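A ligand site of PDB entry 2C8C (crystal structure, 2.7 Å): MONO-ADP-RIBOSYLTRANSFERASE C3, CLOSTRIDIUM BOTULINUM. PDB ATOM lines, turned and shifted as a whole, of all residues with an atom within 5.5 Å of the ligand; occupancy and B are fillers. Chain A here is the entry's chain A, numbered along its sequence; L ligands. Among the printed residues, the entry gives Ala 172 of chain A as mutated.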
ATOM      1  N   TYR A  39       2.802 -20.250 -15.069  1.00  0.00           N
ATOM      2  CA  TYR A  39       2.423 -20.738 -16.400  1.00  0.00           C
ATOM      3  C   TYR A  39       2.962 -19.829 -17.472  1.00  0.00           C
ATOM      4  O   TYR A  39       3.372 -20.268 -18.524  1.00  0.00           O
ATOM      5  CB  TYR A  39       0.904 -20.874 -16.562  1.00  0.00           C
ATOM      6  CG  TYR A  39       0.524 -21.076 -18.013  1.00  0.00           C
ATOM      7  CD1 TYR A  39       0.090 -20.014 -18.783  1.00  0.00           C
ATOM      8  CD2 TYR A  39       0.646 -22.317 -18.621  1.00  0.00           C
ATOM      9  CE1 TYR A  39      -0.244 -20.165 -20.128  1.00  0.00           C
ATOM     10  CE2 TYR A  39       0.304 -22.486 -19.980  1.00  0.00           C
ATOM     11  CZ  TYR A  39      -0.123 -21.393 -20.731  1.00  0.00           C
ATOM     12  OH  TYR A  39      -0.449 -21.529 -22.071  1.00  0.00           O
ATOM     13  N   THR A  40       2.938 -18.532 -17.213  1.00  0.00           N
ATOM     14  CA  THR A  40       3.402 -17.626 -18.235  1.00  0.00           C
ATOM     15  C   THR A  40       4.922 -17.716 -18.395  1.00  0.00           C
ATOM     16  O   THR A  40       5.433 -17.481 -19.487  1.00  0.00           O
ATOM     17  CB  THR A  40       2.891 -16.191 -17.974  1.00  0.00           C
ATOM     18  OG1 THR A  40       3.294 -15.743 -16.682  1.00  0.00           O
ATOM     19  CG2 THR A  40       1.385 -16.186 -17.911  1.00  0.00           C
ATOM     20  N   LYS A  41       5.618 -18.077 -17.321  1.00  0.00           N
ATOM     21  CA  LYS A  41       7.055 -18.291 -17.331  1.00  0.00           C
ATOM     22  C   LYS A  41       7.390 -19.645 -17.933  1.00  0.00           C
ATOM     23  O   LYS A  41       8.545 -19.909 -18.226  1.00  0.00           O
ATOM     24  CB  LYS A  41       7.642 -18.295 -15.913  1.00  0.00           C
ATOM     25  CG  LYS A  41       7.540 -16.994 -15.093  1.00  0.00           C
ATOM     26  CD  LYS A  41       8.101 -17.136 -13.642  1.00  0.00           C
ATOM     27  CE  LYS A  41       8.069 -15.792 -12.908  1.00  0.00           C
ATOM     28  NZ  LYS A  41       8.210 -15.863 -11.389  1.00  0.00           N
ATOM     29  N   ALA A  43       5.064 -21.837 -20.171  1.00  0.00           N
ATOM     30  CA  ALA A  43       3.953 -22.356 -20.923  1.00  0.00           C
ATOM     31  C   ALA A  43       4.346 -23.463 -21.859  1.00  0.00           C
ATOM     32  O   ALA A  43       3.595 -24.426 -22.018  1.00  0.00           O
ATOM     33  CB  ALA A  43       3.291 -21.249 -21.695  1.00  0.00           C
ATOM     34  N   SER A  44       5.469 -23.341 -22.522  1.00  0.00           N
ATOM     35  CA  SER A  44       5.758 -24.241 -23.626  1.00  0.00           C
ATOM     36  C   SER A  44       6.220 -25.586 -23.082  1.00  0.00           C
ATOM     37  O   SER A  44       5.981 -26.637 -23.673  1.00  0.00           O
ATOM     38  CB  SER A  44       6.765 -23.616 -24.634  1.00  0.00           C
ATOM     39  OG  SER A  44       7.973 -23.267 -23.974  1.00  0.00           O
ATOM     40  N   ASN A  47       2.561 -26.983 -21.709  1.00  0.00           N
ATOM     41  CA  ASN A  47       1.722 -27.346 -22.820  1.00  0.00           C
ATOM     42  C   ASN A  47       2.326 -28.502 -23.602  1.00  0.00           C
ATOM     43  O   ASN A  47       1.615 -29.259 -24.196  1.00  0.00           O
ATOM     44  CB  ASN A  47       1.444 -26.140 -23.710  1.00  0.00           C
ATOM     45  CG  ASN A  47       0.407 -25.215 -23.109  1.00  0.00           C
ATOM     46  OD1 ASN A  47      -0.407 -25.653 -22.315  1.00  0.00           O
ATOM     47  ND2 ASN A  47       0.421 -23.962 -23.459  1.00  0.00           N
ATOM     48  N   GLY A  48       3.646 -28.642 -23.589  1.00  0.00           N
ATOM     49  CA  GLY A  48       4.323 -29.633 -24.397  1.00  0.00           C
ATOM     50  C   GLY A  48       4.295 -31.001 -23.777  1.00  0.00           C
ATOM     51  O   GLY A  48       4.070 -31.970 -24.486  1.00  0.00           O
ATOM     52  N   ARG A  51       0.771 -32.239 -24.416  1.00  0.00           N
ATOM     53  CA  ARG A  51       0.649 -32.786 -25.775  1.00  0.00           C
ATOM     54  C   ARG A  51       1.230 -34.164 -25.903  1.00  0.00           C
ATOM     55  O   ARG A  51       0.663 -35.041 -26.547  1.00  0.00           O
ATOM     56  CB  ARG A  51       1.334 -31.874 -26.772  1.00  0.00           C
ATOM     57  CG  ARG A  51       0.592 -30.598 -27.013  1.00  0.00           C
ATOM     58  CD  ARG A  51       1.023 -29.836 -28.256  1.00  0.00           C
ATOM     59  NE  ARG A  51       0.787 -28.404 -28.098  1.00  0.00           N
ATOM     60  CZ  ARG A  51       1.625 -27.567 -27.501  1.00  0.00           C
ATOM     61  NH1 ARG A  51       1.285 -26.303 -27.390  1.00  0.00           N
ATOM     62  NH2 ARG A  51       2.793 -27.960 -27.038  1.00  0.00           N
ATOM     63  N   PHE A  87      -7.102 -13.679 -30.530  1.00  0.00           N
ATOM     64  CA  PHE A  87      -6.103 -13.790 -31.588  1.00  0.00           C
ATOM     65  C   PHE A  87      -4.877 -14.507 -31.092  1.00  0.00           C
ATOM     66  O   PHE A  87      -4.539 -14.453 -29.924  1.00  0.00           O
ATOM     67  CB  PHE A  87      -5.659 -12.426 -32.086  1.00  0.00           C
ATOM     68  CG  PHE A  87      -6.718 -11.645 -32.813  1.00  0.00           C
ATOM     69  CD1 PHE A  87      -7.720 -10.972 -32.085  1.00  0.00           C
ATOM     70  CD2 PHE A  87      -6.723 -11.572 -34.191  1.00  0.00           C
ATOM     71  CE1 PHE A  87      -8.707 -10.262 -32.726  1.00  0.00           C
ATOM     72  CE2 PHE A  87      -7.720 -10.841 -34.860  1.00  0.00           C
ATOM     73  CZ  PHE A  87      -8.728 -10.176 -34.119  1.00  0.00           C
ATOM     74  N   ARG A  88      -4.172 -15.147 -32.014  1.00  0.00           N
ATOM     75  CA  ARG A  88      -3.077 -16.030 -31.659  1.00  0.00           C
ATOM     76  C   ARG A  88      -2.125 -16.195 -32.833  1.00  0.00           C
ATOM     77  O   ARG A  88      -2.562 -16.262 -33.988  1.00  0.00           O
ATOM     78  CB  ARG A  88      -3.663 -17.383 -31.262  1.00  0.00           C
ATOM     79  CG  ARG A  88      -2.730 -18.258 -30.545  1.00  0.00           C
ATOM     80  CD  ARG A  88      -3.106 -19.716 -30.542  1.00  0.00           C
ATOM     81  NE  ARG A  88      -1.902 -20.532 -30.456  1.00  0.00           N
ATOM     82  CZ  ARG A  88      -1.081 -20.555 -29.423  1.00  0.00           C
ATOM     83  NH1 ARG A  88      -1.315 -19.828 -28.353  1.00  0.00           N
ATOM     84  NH2 ARG A  88      -0.018 -21.334 -29.459  1.00  0.00           N
ATOM     85  N   GLY A  89      -0.840 -16.270 -32.553  1.00  0.00           N
ATOM     86  CA  GLY A  89       0.154 -16.527 -33.588  1.00  0.00           C
ATOM     87  C   GLY A  89       0.884 -17.855 -33.359  1.00  0.00           C
ATOM     88  O   GLY A  89       1.134 -18.249 -32.208  1.00  0.00           O
ATOM     89  N   ASP A  90       1.229 -18.538 -34.454  1.00  0.00           N
ATOM     90  CA  ASP A  90       1.886 -19.834 -34.382  1.00  0.00           C
ATOM     91  C   ASP A  90       2.997 -19.954 -35.402  1.00  0.00           C
ATOM     92  O   ASP A  90       3.044 -19.259 -36.411  1.00  0.00           O
ATOM     93  CB  ASP A  90       0.894 -20.941 -34.693  1.00  0.00           C
ATOM     94  CG  ASP A  90      -0.137 -21.104 -33.635  1.00  0.00           C
ATOM     95  OD1 ASP A  90       0.264 -21.562 -32.535  1.00  0.00           O
ATOM     96  OD2 ASP A  90      -1.361 -20.829 -33.835  1.00  0.00           O
ATOM     97  N   ASP A  91       3.856 -20.918 -35.150  1.00  0.00           N
ATOM     98  CA  ASP A  91       4.928 -21.211 -36.070  1.00  0.00           C
ATOM     99  C   ASP A  91       4.535 -22.437 -36.904  1.00  0.00           C
ATOM    100  O   ASP A  91       3.561 -23.134 -36.579  1.00  0.00           O
ATOM    101  CB  ASP A  91       6.190 -21.450 -35.253  1.00  0.00           C
ATOM    102  CG  ASP A  91       6.680 -20.208 -34.571  1.00  0.00           C
ATOM    103  OD1 ASP A  91       6.340 -19.077 -35.042  1.00  0.00           O
ATOM    104  OD2 ASP A  91       7.403 -20.262 -33.551  1.00  0.00           O
ATOM    105  N   ALA A  93       5.354 -25.596 -37.153  1.00  0.00           N
ATOM    106  CA  ALA A  93       5.085 -26.889 -36.502  1.00  0.00           C
ATOM    107  C   ALA A  93       3.624 -27.059 -36.011  1.00  0.00           C
ATOM    108  O   ALA A  93       3.168 -28.176 -35.702  1.00  0.00           O
ATOM    109  CB  ALA A  93       6.096 -27.144 -35.318  1.00  0.00           C
ATOM    110  N   TYR A  94       2.911 -25.933 -35.960  1.00  0.00           N
ATOM    111  CA  TYR A  94       1.509 -25.895 -35.520  1.00  0.00           C
ATOM    112  C   TYR A  94       0.680 -26.749 -36.412  1.00  0.00           C
ATOM    113  O   TYR A  94      -0.245 -27.380 -35.944  1.00  0.00           O
ATOM    114  CB  TYR A  94       0.971 -24.470 -35.510  1.00  0.00           C
ATOM    115  CG  TYR A  94      -0.528 -24.349 -35.309  1.00  0.00           C
ATOM    116  CD1 TYR A  94      -1.104 -24.511 -34.059  1.00  0.00           C
ATOM    117  CD2 TYR A  94      -1.357 -24.086 -36.370  1.00  0.00           C
ATOM    118  CE1 TYR A  94      -2.488 -24.406 -33.871  1.00  0.00           C
ATOM    119  CE2 TYR A  94      -2.742 -23.988 -36.201  1.00  0.00           C
ATOM    120  CZ  TYR A  94      -3.317 -24.150 -34.950  1.00  0.00           C
ATOM    121  OH  TYR A  94      -4.704 -24.036 -34.830  1.00  0.00           O
ATOM    122  N   ARG A 127     -10.193 -29.695 -34.201  1.00  0.00           N
ATOM    123  CA  ARG A 127      -8.877 -29.893 -33.705  1.00  0.00           C
ATOM    124  C   ARG A 127      -8.960 -29.941 -32.190  1.00  0.00           C
ATOM    125  O   ARG A 127      -9.665 -29.131 -31.558  1.00  0.00           O
ATOM    126  CB  ARG A 127      -7.994 -28.755 -34.170  1.00  0.00           C
ATOM    127  CG  ARG A 127      -6.566 -28.925 -33.778  1.00  0.00           C
ATOM    128  CD  ARG A 127      -5.597 -28.501 -34.856  1.00  0.00           C
ATOM    129  NE  ARG A 127      -4.239 -28.607 -34.355  1.00  0.00           N
ATOM    130  CZ  ARG A 127      -3.185 -27.969 -34.845  1.00  0.00           C
ATOM    131  NH1 ARG A 127      -3.296 -27.139 -35.872  1.00  0.00           N
ATOM    132  NH2 ARG A 127      -2.005 -28.153 -34.269  1.00  0.00           N
ATOM    133  N   GLU A 129      -6.820 -29.651 -28.796  1.00  0.00           N
ATOM    134  CA  GLU A 129      -5.570 -29.198 -28.243  1.00  0.00           C
ATOM    135  C   GLU A 129      -5.440 -29.682 -26.791  1.00  0.00           C
ATOM    136  O   GLU A 129      -6.244 -29.377 -25.927  1.00  0.00           O
ATOM    137  CB  GLU A 129      -5.434 -27.667 -28.407  1.00  0.00           C
ATOM    138  CG  GLU A 129      -4.102 -27.031 -27.993  1.00  0.00           C
ATOM    139  CD  GLU A 129      -2.833 -27.847 -28.352  1.00  0.00           C
ATOM    140  OE1 GLU A 129      -1.938 -27.982 -27.475  1.00  0.00           O
ATOM    141  OE2 GLU A 129      -2.757 -28.339 -29.500  1.00  0.00           O
ATOM    142  N   TYR A 132      -3.012 -25.854 -22.750  1.00  0.00           N
ATOM    143  CA  TYR A 132      -3.701 -24.572 -22.653  1.00  0.00           C
ATOM    144  C   TYR A 132      -3.557 -23.759 -23.927  1.00  0.00           C
ATOM    145  O   TYR A 132      -2.692 -24.010 -24.720  1.00  0.00           O
ATOM    146  CB  TYR A 132      -3.226 -23.775 -21.457  1.00  0.00           C
ATOM    147  CG  TYR A 132      -3.509 -24.487 -20.189  1.00  0.00           C
ATOM    148  CD1 TYR A 132      -4.758 -24.435 -19.616  1.00  0.00           C
ATOM    149  CD2 TYR A 132      -2.552 -25.277 -19.592  1.00  0.00           C
ATOM    150  CE1 TYR A 132      -5.025 -25.122 -18.476  1.00  0.00           C
ATOM    151  CE2 TYR A 132      -2.819 -25.964 -18.453  1.00  0.00           C
ATOM    152  CZ  TYR A 132      -4.056 -25.881 -17.892  1.00  0.00           C
ATOM    153  OH  TYR A 132      -4.337 -26.587 -16.734  1.00  0.00           O
ATOM    154  N   SER A 134      -3.055 -19.879 -25.120  1.00  0.00           N
ATOM    155  CA  SER A 134      -2.787 -18.479 -24.836  1.00  0.00           C
ATOM    156  C   SER A 134      -3.221 -17.671 -26.036  1.00  0.00           C
ATOM    157  O   SER A 134      -2.971 -18.074 -27.134  1.00  0.00           O
ATOM    158  CB  SER A 134      -1.301 -18.285 -24.609  1.00  0.00           C
ATOM    159  OG  SER A 134      -0.852 -18.961 -23.450  1.00  0.00           O
ATOM    160  N   THR A 135      -3.886 -16.548 -25.816  1.00  0.00           N
ATOM    161  CA  THR A 135      -4.377 -15.702 -26.929  1.00  0.00           C
ATOM    162  C   THR A 135      -4.264 -14.232 -26.542  1.00  0.00           C
ATOM    163  O   THR A 135      -3.851 -13.915 -25.438  1.00  0.00           O
ATOM    164  CB  THR A 135      -5.856 -16.000 -27.267  1.00  0.00           C
ATOM    165  OG1 THR A 135      -6.620 -15.914 -26.066  1.00  0.00           O
ATOM    166  CG2 THR A 135      -6.054 -17.421 -27.666  1.00  0.00           C
ATOM    167  N   SER A 136      -4.666 -13.347 -27.430  1.00  0.00           N
ATOM    168  CA  SER A 136      -4.655 -11.908 -27.143  1.00  0.00           C
ATOM    169  C   SER A 136      -5.972 -11.269 -27.539  1.00  0.00           C
ATOM    170  O   SER A 136      -6.709 -11.798 -28.368  1.00  0.00           O
ATOM    171  CB  SER A 136      -3.525 -11.228 -27.880  1.00  0.00           C
ATOM    172  OG  SER A 136      -2.301 -11.769 -27.471  1.00  0.00           O
ATOM    173  N   PHE A 143       3.397 -11.151 -31.503  1.00  0.00           N
ATOM    174  CA  PHE A 143       2.969 -12.436 -32.045  1.00  0.00           C
ATOM    175  C   PHE A 143       2.367 -12.308 -33.445  1.00  0.00           C
ATOM    176  O   PHE A 143       2.018 -13.313 -34.067  1.00  0.00           O
ATOM    177  CB  PHE A 143       1.987 -13.094 -31.059  1.00  0.00           C
ATOM    178  CG  PHE A 143       2.647 -13.547 -29.753  1.00  0.00           C
ATOM    179  CD1 PHE A 143       2.438 -12.849 -28.568  1.00  0.00           C
ATOM    180  CD2 PHE A 143       3.493 -14.648 -29.716  1.00  0.00           C
ATOM    181  CE1 PHE A 143       3.040 -13.259 -27.371  1.00  0.00           C
ATOM    182  CE2 PHE A 143       4.103 -15.047 -28.524  1.00  0.00           C
ATOM    183  CZ  PHE A 143       3.881 -14.361 -27.365  1.00  0.00           C
ATOM    184  N   ARG A 146       4.622 -13.693 -36.521  1.00  0.00           N
ATOM    185  CA  ARG A 146       4.537 -15.136 -36.823  1.00  0.00           C
ATOM    186  C   ARG A 146       3.747 -15.510 -38.094  1.00  0.00           C
ATOM    187  O   ARG A 146       2.750 -14.870 -38.438  1.00  0.00           O
ATOM    188  CB  ARG A 146       3.894 -15.870 -35.639  1.00  0.00           C
ATOM    189  CG  ARG A 146       4.659 -15.796 -34.360  1.00  0.00           C
ATOM    190  CD  ARG A 146       4.403 -16.952 -33.429  1.00  0.00           C
ATOM    191  NE  ARG A 146       5.217 -16.895 -32.201  1.00  0.00           N
ATOM    192  CZ  ARG A 146       5.069 -17.712 -31.149  1.00  0.00           C
ATOM    193  NH1 ARG A 146       4.177 -18.682 -31.156  1.00  0.00           N
ATOM    194  NH2 ARG A 146       5.841 -17.579 -30.075  1.00  0.00           N
ATOM    195  N   SER A 167       0.653 -11.652 -15.532  1.00  0.00           N
ATOM    196  CA  SER A 167       1.659 -12.289 -16.380  1.00  0.00           C
ATOM    197  C   SER A 167       3.035 -11.772 -16.054  1.00  0.00           C
ATOM    198  O   SER A 167       3.210 -10.591 -15.754  1.00  0.00           O
ATOM    199  CB  SER A 167       1.398 -12.027 -17.856  1.00  0.00           C
ATOM    200  OG  SER A 167       2.359 -12.684 -18.693  1.00  0.00           O
ATOM    201  N   PHE A 169       5.189 -11.412 -18.329  1.00  0.00           N
ATOM    202  CA  PHE A 169       5.535 -10.679 -19.555  1.00  0.00           C
ATOM    203  C   PHE A 169       4.531  -9.611 -19.987  1.00  0.00           C
ATOM    204  O   PHE A 169       3.375  -9.668 -19.636  1.00  0.00           O
ATOM    205  CB  PHE A 169       5.781 -11.693 -20.699  1.00  0.00           C
ATOM    206  CG  PHE A 169       6.944 -12.607 -20.423  1.00  0.00           C
ATOM    207  CD1 PHE A 169       6.744 -13.879 -19.891  1.00  0.00           C
ATOM    208  CD2 PHE A 169       8.252 -12.155 -20.624  1.00  0.00           C
ATOM    209  CE1 PHE A 169       7.814 -14.694 -19.604  1.00  0.00           C
ATOM    210  CE2 PHE A 169       9.327 -12.985 -20.320  1.00  0.00           C
ATOM    211  CZ  PHE A 169       9.112 -14.245 -19.803  1.00  0.00           C
ATOM    212  N   ALA A 172       1.055  -8.276 -24.141  1.00  0.00           N
ATOM    213  CA  ALA A 172       0.331  -9.390 -24.801  1.00  0.00           C
ATOM    214  C   ALA A 172      -1.213  -9.333 -24.777  1.00  0.00           C
ATOM    215  O   ALA A 172      -1.874 -10.096 -25.458  1.00  0.00           O
ATOM    216  CB  ALA A 172       0.814 -10.724 -24.242  1.00  0.00           C
ATOM    217  N   GLU A 174      -3.175 -10.636 -22.703  1.00  0.00           N
ATOM    218  CA  GLU A 174      -3.343 -12.089 -22.695  1.00  0.00           C
ATOM    219  C   GLU A 174      -4.686 -12.616 -22.098  1.00  0.00           C
ATOM    220  O   GLU A 174      -5.037 -12.358 -20.927  1.00  0.00           O
ATOM    221  CB  GLU A 174      -2.107 -12.768 -22.010  1.00  0.00           C
ATOM    222  CG  GLU A 174      -2.063 -14.301 -22.147  1.00  0.00           C
ATOM    223  CD  GLU A 174      -0.719 -14.940 -21.710  1.00  0.00           C
ATOM    224  OE1 GLU A 174       0.198 -14.191 -21.267  1.00  0.00           O
ATOM    225  OE2 GLU A 174      -0.592 -16.197 -21.787  1.00  0.00           O
HETATM  226  P1  LIG L   1       2.549 -22.857 -27.003  1.00  0.00           P
HETATM  227  O1  LIG L   1       1.072 -22.650 -27.191  1.00  0.00           O
HETATM  228  O2  LIG L   1       2.756 -23.957 -25.944  1.00  0.00           O
HETATM  229  O3  LIG L   1       3.309 -23.097 -28.446  1.00  0.00           O
HETATM  230  C1  LIG L   1       4.724 -23.073 -28.513  1.00  0.00           C
HETATM  231  C2  LIG L   1       5.217 -23.471 -29.909  1.00  0.00           C
HETATM  232  O4  LIG L   1       4.636 -24.695 -30.345  1.00  0.00           O
HETATM  233  C3  LIG L   1       4.840 -22.432 -30.943  1.00  0.00           C
HETATM  234  O5  LIG L   1       5.813 -22.513 -31.990  1.00  0.00           O
HETATM  235  C4  LIG L   1       3.491 -22.876 -31.450  1.00  0.00           C
HETATM  236  O6  LIG L   1       3.208 -22.261 -32.694  1.00  0.00           O
HETATM  237  C5  LIG L   1       3.711 -24.414 -31.404  1.00  0.00           C
HETATM  238  N1  LIG L   1       2.497 -25.233 -31.199  1.00  0.00           N
HETATM  239  C6  LIG L   1       1.281 -24.821 -30.690  1.00  0.00           C
HETATM  240  N2  LIG L   1       0.433 -25.885 -30.685  1.00  0.00           N
HETATM  241  C7  LIG L   1       1.106 -26.966 -31.190  1.00  0.00           C
HETATM  242  C8  LIG L   1       0.684 -28.289 -31.417  1.00  0.00           C
HETATM  243  N3  LIG L   1      -0.586 -28.642 -31.095  1.00  0.00           N
HETATM  244  N4  LIG L   1       1.599 -29.186 -31.966  1.00  0.00           N
HETATM  245  C9  LIG L   1       2.878 -28.769 -32.270  1.00  0.00           C
HETATM  246  N5  LIG L   1       3.281 -27.466 -32.055  1.00  0.00           N
HETATM  247  C10 LIG L   1       2.394 -26.570 -31.529  1.00  0.00           C
HETATM  248  O7  LIG L   1       3.332 -21.518 -26.496  1.00  0.00           O
HETATM  249  P2  LIG L   1       3.197 -20.069 -27.253  1.00  0.00           P
HETATM  250  O8  LIG L   1       1.757 -19.644 -27.355  1.00  0.00           O
HETATM  251  O9  LIG L   1       4.098 -19.919 -28.426  1.00  0.00           O
HETATM  252  O10 LIG L   1       3.926 -19.077 -26.204  1.00  0.00           O
HETATM  253  C11 LIG L   1       3.302 -18.729 -24.994  1.00  0.00           C
HETATM  254  C12 LIG L   1       4.064 -17.564 -24.345  1.00  0.00           C
HETATM  255  O11 LIG L   1       3.624 -16.378 -24.980  1.00  0.00           O
HETATM  256  C13 LIG L   1       3.556 -17.494 -22.930  1.00  0.00           C
HETATM  257  O12 LIG L   1       4.384 -16.612 -22.199  1.00  0.00           O
HETATM  258  C14 LIG L   1       2.185 -16.861 -23.149  1.00  0.00           C
HETATM  259  O13 LIG L   1       1.840 -15.991 -22.115  1.00  0.00           O
HETATM  260  C15 LIG L   1       2.402 -15.942 -24.340  1.00  0.00           C
HETATM  261  N6  LIG L   1       1.311 -15.598 -25.305  1.00  0.00           N
HETATM  262  C16 LIG L   1       1.286 -16.099 -26.582  1.00  0.00           C
HETATM  263  C17 LIG L   1       0.279 -15.698 -27.456  1.00  0.00           C
HETATM  264  C18 LIG L   1       0.234 -16.231 -28.837  1.00  0.00           C
HETATM  265  O14 LIG L   1      -0.744 -15.723 -29.711  1.00  0.00           O
HETATM  266  N7  LIG L   1       1.115 -17.149 -29.236  1.00  0.00           N
HETATM  267  C19 LIG L   1      -0.670 -14.760 -27.070  1.00  0.00           C
HETATM  268  C20 LIG L   1      -0.623 -14.225 -25.808  1.00  0.00           C
HETATM  269  C21 LIG L   1       0.371 -14.661 -24.930  1.00  0.00           C
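A nitrogen (N3) of the ligand sits at hydrogen-bond distance from the side-chain carboxylate (OE2) of Glu 129.
An oxygen (O6) of the ligand sits at hydrogen-bond distance from the backbone NH of Asp 91, 2.9 Å away.
N of Gly 89 sits at hydrogen-bond distance from O14 of the ligand.
O1 of the ligand is in salt-bridge range of NH2 of Arg 88.
The backbone carbonyl oxygen of Gly 89 sits at hydrogen-bond distance from a nitrogen (N7) of the ligand.
ND2 of Asn 47 sits close to O2 of the ligand (3.4 Å).
The side-chain carboxylate (OD2) of Asp 91 sits at hydrogen-bond distance from an oxygen (O5) of the ligand, 3.2 Å away.
O9 of the ligand lies within salt-bridge range of NH1 of Arg 146 (3.0 Å).
The backbone carbonyl oxygen of Thr 40 lies within hydrogen-bond range of an oxygen (O12) of the ligand (3.0 Å).
The side-chain carboxylate (OD1) of Asp 90 sits at hydrogen-bond distance from an oxygen (O6) of the ligand (3.0 Å).
An oxygen (O13) of the ligand lies within hydrogen-bond range of the side-chain carboxylate of Glu 174, at 2.5 Å.
The guanidinium group (NH1) of Arg 51 lies within salt-bridge range of an oxygen (O2) of the ligand.
ND2 of Asn 47 lies within hydrogen-bond range of OH of Tyr 39.
The side-chain hydroxyl (OH) of Tyr 39 is in hydrogen-bond range of the side-chain hydroxyl (OG) of Ser 134, 2.9 Å away.
The backbone carbonyl oxygen (O) of Ser 134 lies within hydrogen-bond range of the guanidinium group (NH1) of Arg 88 (2.7 Å).
The side-chain carboxylate (OD1) of Asp 91 is in salt-bridge range of the guanidinium group (NE) of Arg 146 (3.8 Å).
NH2 of Arg 88 is in salt-bridge range of OD1 of Asp 90.
OE2 of Glu 174 lies within hydrogen-bond range of OG of Ser 134 (3.2 Å).
The guanidinium group (NH1) of Arg 146 is in hydrogen-bond range of the backbone carbonyl oxygen (O) of Gly 89 (3.2 Å).
The backbone carbonyl oxygen (O) of Tyr 94 is in hydrogen-bond range of the guanidinium group (NH2) of Arg 127 (2.5 Å).
Ala 43 touches the ligand.
Ser 44 touches the ligand (CA to O2, 3.8 Å).
O of Ala 93 touches C9 of the ligand, at 3.5 Å.
Tyr 94 touches the ligand (CD1 to N2, 3.95 Å).
Arg 127 touches the ligand.
Ser 134 touches the ligand.
Thr 135 touches the ligand (O to C20, 3.3 Å).
Ser 136 touches the ligand.
Phe 143 touches the ligand.
Hydrophobic or aromatic side chains that line the ligand: Ala 43, Tyr 94 and Phe 143.
Of the 27 residues printed, 19 come within 4 Å of the ligand.
The nearest printed residue that does not touch the ligand is Phe 87 (4.01 Å).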
